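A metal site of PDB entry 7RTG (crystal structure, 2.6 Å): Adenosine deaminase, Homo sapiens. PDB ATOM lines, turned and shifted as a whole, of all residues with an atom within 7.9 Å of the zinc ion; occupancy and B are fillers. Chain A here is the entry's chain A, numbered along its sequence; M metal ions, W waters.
Water W1 lies within hydrogen-bond range of the side-chain carboxylate (OD2) of Asp 295 (2.4 Å), the side-chain carboxylate (OE2) of Glu 217 (3.2 Å) and a ring nitrogen (NE2) of His 238 (3.5 Å).
NE2 of His 15 binds the zinc ion (2.0 Å).
The zinc ion is bound by a ring nitrogen (NE2) of His 17 (2.1 Å).
A ring nitrogen (NE2) of His 214 binds the zinc ion (2.1 Å).
OD1 of Asp 295 binds the zinc ion (2.1 Å).
Water W1 binds the zinc ion (2.5 Å).
Residues that only touch the zinc ion: His 238 (3.2 Å).
Within 4 Å of the zinc ion: His 15, His 17, His 214, His 238 and Asp 295.
The nearest printed residue that does not touch the zinc ion is Arg 101 (5.0 Å).
The side-chain carboxylate (OE1) of Glu 260 lies within hydrogen-bond range of a ring nitrogen (ND1) of His 15.
N of His 15 lies within hydrogen-bond range of OD1 of Asn 293 (2.8 Å).
A ring nitrogen (ND1) of His 214 lies within hydrogen-bond range of the side-chain carboxylate (OD2) of Asp 181, at 3.0 Å.
N of His 214 lies within hydrogen-bond range of O of Leu 182 (3.2 Å).
The side-chain carboxylate (OD2) of Asp 295 is in hydrogen-bond range of a ring nitrogen (NE2) of His 238, 3.3 Å away.
The side-chain hydroxyl of Ser 265 lies within hydrogen-bond range of the side-chain carboxylate of Asp 295 (3.1 Å).
The backbone carbonyl oxygen (O) of His 238 is in hydrogen-bond range of the backbone NH (N) of Glu 217 (3.3 Å).
N of His 238 sits at hydrogen-bond distance from O of Glu 260 (3.3 Å).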
ATOM      1  N   HIS A  15     -34.853  19.117  12.737  1.00  0.00           N
ATOM      2  CA  HIS A  15     -33.550  18.500  12.505  1.00  0.00           C
ATOM      3  C   HIS A  15     -33.514  17.120  13.160  1.00  0.00           C
ATOM      4  O   HIS A  15     -33.186  16.988  14.339  1.00  0.00           O
ATOM      5  CB  HIS A  15     -32.429  19.397  13.019  1.00  0.00           C
ATOM      6  CG  HIS A  15     -31.053  18.952  12.622  1.00  0.00           C
ATOM      7  ND1 HIS A  15     -30.004  19.827  12.501  1.00  0.00           N
ATOM      8  CD2 HIS A  15     -30.565  17.718  12.336  1.00  0.00           C
ATOM      9  CE1 HIS A  15     -28.920  19.156  12.150  1.00  0.00           C
ATOM     10  NE2 HIS A  15     -29.234  17.882  12.040  1.00  0.00           N
ATOM     11  N   VAL A  16     -33.838  16.087  12.380  1.00  0.00           N
ATOM     12  CA  VAL A  16     -33.653  14.709  12.824  1.00  0.00           C
ATOM     13  C   VAL A  16     -33.460  13.847  11.579  1.00  0.00           C
ATOM     14  O   VAL A  16     -34.175  14.003  10.581  1.00  0.00           O
ATOM     15  CB  VAL A  16     -34.841  14.220  13.684  1.00  0.00           C
ATOM     16  CG1 VAL A  16     -36.162  14.524  13.013  1.00  0.00           C
ATOM     17  CG2 VAL A  16     -34.719  12.730  13.988  1.00  0.00           C
ATOM     18  N   HIS A  17     -32.477  12.946  11.633  1.00  0.00           N
ATOM     19  CA  HIS A  17     -32.111  12.139  10.487  1.00  0.00           C
ATOM     20  C   HIS A  17     -32.834  10.798  10.531  1.00  0.00           C
ATOM     21  O   HIS A  17     -32.911  10.148  11.581  1.00  0.00           O
ATOM     22  CB  HIS A  17     -30.596  11.903  10.447  1.00  0.00           C
ATOM     23  CG  HIS A  17     -29.786  13.166  10.530  1.00  0.00           C
ATOM     24  ND1 HIS A  17     -29.031  13.634   9.472  1.00  0.00           N
ATOM     25  CD2 HIS A  17     -29.593  14.041  11.544  1.00  0.00           C
ATOM     26  CE1 HIS A  17     -28.415  14.751   9.827  1.00  0.00           C
ATOM     27  NE2 HIS A  17     -28.742  15.021  11.078  1.00  0.00           N
ATOM     28  N   PHE A  61     -18.973   9.156  16.257  1.00  0.00           N
ATOM     29  CA  PHE A  61     -20.427   9.063  16.120  1.00  0.00           C
ATOM     30  C   PHE A  61     -20.822   8.643  14.717  1.00  0.00           C
ATOM     31  O   PHE A  61     -21.676   7.756  14.537  1.00  0.00           O
ATOM     32  CB  PHE A  61     -21.077  10.395  16.487  1.00  0.00           C
ATOM     33  CG  PHE A  61     -22.369  10.623  15.784  1.00  0.00           C
ATOM     34  CD1 PHE A  61     -23.506   9.908  16.137  1.00  0.00           C
ATOM     35  CD2 PHE A  61     -22.443  11.552  14.753  1.00  0.00           C
ATOM     36  CE1 PHE A  61     -24.682  10.120  15.474  1.00  0.00           C
ATOM     37  CE2 PHE A  61     -23.625  11.766  14.097  1.00  0.00           C
ATOM     38  CZ  PHE A  61     -24.750  11.054  14.458  1.00  0.00           C
ATOM     39  N   ARG A 101     -34.596  14.168   7.570  1.00  0.00           N
ATOM     40  CA  ARG A 101     -33.579  14.265   6.550  1.00  0.00           C
ATOM     41  C   ARG A 101     -32.784  12.975   6.431  1.00  0.00           C
ATOM     42  O   ARG A 101     -32.636  12.220   7.399  1.00  0.00           O
ATOM     43  CB  ARG A 101     -32.628  15.435   6.829  1.00  0.00           C
ATOM     44  CG  ARG A 101     -31.895  15.331   8.157  1.00  0.00           C
ATOM     45  CD  ARG A 101     -31.142  16.622   8.471  1.00  0.00           C
ATOM     46  NE  ARG A 101     -32.051  17.760   8.629  1.00  0.00           N
ATOM     47  CZ  ARG A 101     -31.644  19.011   8.827  1.00  0.00           C
ATOM     48  NH1 ARG A 101     -30.359  19.289   8.897  1.00  0.00           N
ATOM     49  NH2 ARG A 101     -32.541  19.981   8.969  1.00  0.00           N
ATOM     50  N   CYS A 153     -30.158  14.806   1.907  1.00  0.00           N
ATOM     51  CA  CYS A 153     -28.837  15.158   2.428  1.00  0.00           C
ATOM     52  C   CYS A 153     -27.766  15.095   1.343  1.00  0.00           C
ATOM     53  O   CYS A 153     -27.733  14.165   0.526  1.00  0.00           O
ATOM     54  CB  CYS A 153     -28.445  14.218   3.556  1.00  0.00           C
ATOM     55  SG  CYS A 153     -29.169  14.592   5.173  1.00  0.00           S
ATOM     56  N   ASP A 181     -30.078  19.558   2.340  1.00  0.00           N
ATOM     57  CA  ASP A 181     -29.168  19.670   3.476  1.00  0.00           C
ATOM     58  C   ASP A 181     -27.753  19.333   3.024  1.00  0.00           C
ATOM     59  O   ASP A 181     -27.533  18.790   1.945  1.00  0.00           O
ATOM     60  CB  ASP A 181     -29.602  18.752   4.628  1.00  0.00           C
ATOM     61  CG  ASP A 181     -28.878  19.061   5.925  1.00  0.00           C
ATOM     62  OD1 ASP A 181     -28.644  20.255   6.206  1.00  0.00           O
ATOM     63  OD2 ASP A 181     -28.533  18.116   6.661  1.00  0.00           O
ATOM     64  N   LEU A 182     -26.788  19.692   3.882  1.00  0.00           N
ATOM     65  CA  LEU A 182     -25.383  19.328   3.699  1.00  0.00           C
ATOM     66  C   LEU A 182     -24.889  18.760   5.018  1.00  0.00           C
ATOM     67  O   LEU A 182     -24.591  19.515   5.954  1.00  0.00           O
ATOM     68  CB  LEU A 182     -24.557  20.533   3.261  1.00  0.00           C
ATOM     69  CG  LEU A 182     -23.037  20.346   3.262  1.00  0.00           C
ATOM     70  CD1 LEU A 182     -22.606  19.383   2.160  1.00  0.00           C
ATOM     71  CD2 LEU A 182     -22.332  21.685   3.116  1.00  0.00           C
ATOM     72  N   ALA A 183     -24.798  17.440   5.106  1.00  0.00           N
ATOM     73  CA  ALA A 183     -24.447  16.745   6.333  1.00  0.00           C
ATOM     74  C   ALA A 183     -23.086  16.081   6.184  1.00  0.00           C
ATOM     75  O   ALA A 183     -22.341  16.345   5.232  1.00  0.00           O
ATOM     76  CB  ALA A 183     -25.535  15.731   6.698  1.00  0.00           C
ATOM     77  N   GLY A 184     -22.758  15.212   7.140  1.00  0.00           N
ATOM     78  CA  GLY A 184     -21.517  14.478   7.078  1.00  0.00           C
ATOM     79  C   GLY A 184     -20.450  15.009   8.010  1.00  0.00           C
ATOM     80  O   GLY A 184     -20.733  15.535   9.086  1.00  0.00           O
ATOM     81  N   HIS A 214     -25.659  21.792   7.860  1.00  0.00           N
ATOM     82  CA  HIS A 214     -24.948  21.474   9.097  1.00  0.00           C
ATOM     83  C   HIS A 214     -23.701  22.363   9.181  1.00  0.00           C
ATOM     84  O   HIS A 214     -22.768  22.207   8.395  1.00  0.00           O
ATOM     85  CB  HIS A 214     -24.532  19.994   9.140  1.00  0.00           C
ATOM     86  CG  HIS A 214     -25.603  19.062   9.647  1.00  0.00           C
ATOM     87  ND1 HIS A 214     -26.711  18.717   8.909  1.00  0.00           N
ATOM     88  CD2 HIS A 214     -25.703  18.379  10.807  1.00  0.00           C
ATOM     89  CE1 HIS A 214     -27.459  17.875   9.602  1.00  0.00           C
ATOM     90  NE2 HIS A 214     -26.870  17.660  10.768  1.00  0.00           N
ATOM     91  N   GLU A 217     -21.228  22.885  14.212  1.00  0.00           N
ATOM     92  CA  GLU A 217     -21.459  21.807  15.153  1.00  0.00           C
ATOM     93  C   GLU A 217     -20.148  21.337  15.816  1.00  0.00           C
ATOM     94  O   GLU A 217     -20.102  21.124  17.029  1.00  0.00           O
ATOM     95  CB  GLU A 217     -22.163  20.674  14.418  1.00  0.00           C
ATOM     96  CG  GLU A 217     -22.243  19.328  15.066  1.00  0.00           C
ATOM     97  CD  GLU A 217     -22.463  18.256  14.016  1.00  0.00           C
ATOM     98  OE1 GLU A 217     -21.989  18.420  12.869  1.00  0.00           O
ATOM     99  OE2 GLU A 217     -23.176  17.273  14.328  1.00  0.00           O
ATOM    100  N   GLY A 237     -28.009  23.912  10.891  1.00  0.00           N
ATOM    101  CA  GLY A 237     -27.974  22.730  11.727  1.00  0.00           C
ATOM    102  C   GLY A 237     -26.828  22.832  12.708  1.00  0.00           C
ATOM    103  O   GLY A 237     -25.675  22.939  12.284  1.00  0.00           O
ATOM    104  N   HIS A 238     -27.135  22.828  14.006  1.00  0.00           N
ATOM    105  CA  HIS A 238     -26.151  22.960  15.088  1.00  0.00           C
ATOM    106  C   HIS A 238     -25.370  24.278  14.966  1.00  0.00           C
ATOM    107  O   HIS A 238     -24.170  24.292  14.695  1.00  0.00           O
ATOM    108  CB  HIS A 238     -25.137  21.823  15.096  1.00  0.00           C
ATOM    109  CG  HIS A 238     -25.722  20.446  14.972  1.00  0.00           C
ATOM    110  ND1 HIS A 238     -25.477  19.652  13.873  1.00  0.00           N
ATOM    111  CD2 HIS A 238     -26.440  19.695  15.837  1.00  0.00           C
ATOM    112  CE1 HIS A 238     -26.079  18.484  14.042  1.00  0.00           C
ATOM    113  NE2 HIS A 238     -26.664  18.479  15.225  1.00  0.00           N
ATOM    114  N   GLU A 260     -31.084  25.198  14.398  1.00  0.00           N
ATOM    115  CA  GLU A 260     -31.644  23.882  14.707  1.00  0.00           C
ATOM    116  C   GLU A 260     -30.862  23.281  15.866  1.00  0.00           C
ATOM    117  O   GLU A 260     -29.915  22.510  15.674  1.00  0.00           O
ATOM    118  CB  GLU A 260     -31.630  22.994  13.480  1.00  0.00           C
ATOM    119  CG  GLU A 260     -32.349  23.573  12.272  1.00  0.00           C
ATOM    120  CD  GLU A 260     -32.093  22.801  10.982  1.00  0.00           C
ATOM    121  OE1 GLU A 260     -31.249  21.871  10.994  1.00  0.00           O
ATOM    122  OE2 GLU A 260     -32.729  23.132   9.951  1.00  0.00           O
ATOM    123  N   CYS A 262     -29.857  20.971  19.017  1.00  0.00           N
ATOM    124  CA  CYS A 262     -30.012  19.580  19.431  1.00  0.00           C
ATOM    125  C   CYS A 262     -29.238  19.392  20.726  1.00  0.00           C
ATOM    126  O   CYS A 262     -28.069  18.987  20.701  1.00  0.00           O
ATOM    127  CB  CYS A 262     -29.535  18.603  18.355  1.00  0.00           C
ATOM    128  SG  CYS A 262     -30.201  18.918  16.704  1.00  0.00           S
ATOM    129  N   SER A 265     -27.890  15.718  21.707  1.00  0.00           N
ATOM    130  CA  SER A 265     -26.916  15.414  20.663  1.00  0.00           C
ATOM    131  C   SER A 265     -25.639  16.223  20.845  1.00  0.00           C
ATOM    132  O   SER A 265     -24.539  15.696  20.692  1.00  0.00           O
ATOM    133  CB  SER A 265     -27.534  15.684  19.292  1.00  0.00           C
ATOM    134  OG  SER A 265     -26.542  16.125  18.379  1.00  0.00           O
ATOM    135  N   ASN A 293     -34.432  19.730  18.850  1.00  0.00           N
ATOM    136  CA  ASN A 293     -34.490  18.560  18.002  1.00  0.00           C
ATOM    137  C   ASN A 293     -33.722  17.421  18.648  1.00  0.00           C
ATOM    138  O   ASN A 293     -32.964  17.606  19.599  1.00  0.00           O
ATOM    139  CB  ASN A 293     -33.902  18.847  16.607  1.00  0.00           C
ATOM    140  CG  ASN A 293     -34.549  20.042  15.943  1.00  0.00           C
ATOM    141  OD1 ASN A 293     -35.607  19.924  15.313  1.00  0.00           O
ATOM    142  ND2 ASN A 293     -33.922  21.203  16.062  1.00  0.00           N
ATOM    143  N   THR A 294     -33.934  16.216  18.119  1.00  0.00           N
ATOM    144  CA  THR A 294     -33.299  15.002  18.626  1.00  0.00           C
ATOM    145  C   THR A 294     -32.023  14.654  17.883  1.00  0.00           C
ATOM    146  O   THR A 294     -31.185  13.936  18.427  1.00  0.00           O
ATOM    147  CB  THR A 294     -34.255  13.808  18.531  1.00  0.00           C
ATOM    148  OG1 THR A 294     -34.801  13.725  17.218  1.00  0.00           O
ATOM    149  CG2 THR A 294     -35.378  13.940  19.530  1.00  0.00           C
ATOM    150  N   ASP A 295     -31.870  15.118  16.638  1.00  0.00           N
ATOM    151  CA  ASP A 295     -30.825  14.699  15.720  1.00  0.00           C
ATOM    152  C   ASP A 295     -30.993  13.215  15.410  1.00  0.00           C
ATOM    153  O   ASP A 295     -31.698  12.867  14.459  1.00  0.00           O
ATOM    154  CB  ASP A 295     -29.428  15.017  16.269  1.00  0.00           C
ATOM    155  CG  ASP A 295     -28.407  15.368  15.161  1.00  0.00           C
ATOM    156  OD1 ASP A 295     -28.772  15.801  14.042  1.00  0.00           O
ATOM    157  OD2 ASP A 295     -27.198  15.217  15.447  1.00  0.00           O
ATOM    158  N   ASP A 296     -30.395  12.324  16.215  1.00  0.00           N
ATOM    159  CA  ASP A 296     -30.459  10.876  15.970  1.00  0.00           C
ATOM    160  C   ASP A 296     -30.784  10.113  17.258  1.00  0.00           C
ATOM    161  O   ASP A 296     -29.883   9.697  17.986  1.00  0.00           O
ATOM    162  CB  ASP A 296     -29.141  10.367  15.371  1.00  0.00           C
ATOM    163  CG  ASP A 296     -28.701  11.162  14.134  1.00  0.00           C
ATOM    164  OD1 ASP A 296     -29.540  11.786  13.452  1.00  0.00           O
ATOM    165  OD2 ASP A 296     -27.496  11.177  13.841  1.00  0.00           O
ATOM    166  N   PHE A 300     -28.323   8.219  20.038  1.00  0.00           N
ATOM    167  CA  PHE A 300     -28.197   8.939  21.293  1.00  0.00           C
ATOM    168  C   PHE A 300     -29.066   8.353  22.405  1.00  0.00           C
ATOM    169  O   PHE A 300     -29.078   8.902  23.521  1.00  0.00           O
ATOM    170  CB  PHE A 300     -28.532  10.403  21.057  1.00  0.00           C
ATOM    171  CG  PHE A 300     -27.600  11.073  20.094  1.00  0.00           C
ATOM    172  CD1 PHE A 300     -26.246  10.775  20.121  1.00  0.00           C
ATOM    173  CD2 PHE A 300     -28.078  11.938  19.130  1.00  0.00           C
ATOM    174  CE1 PHE A 300     -25.376  11.359  19.240  1.00  0.00           C
ATOM    175  CE2 PHE A 300     -27.196  12.531  18.229  1.00  0.00           C
ATOM    176  CZ  PHE A 300     -25.849  12.243  18.288  1.00  0.00           C
HETATM  177 ZN    ZN M   1     -27.796  16.448  12.247  1.00  0.00          ZN
HETATM  178  O   HOH W   1     -25.793  15.585  13.529  1.00  0.00           O
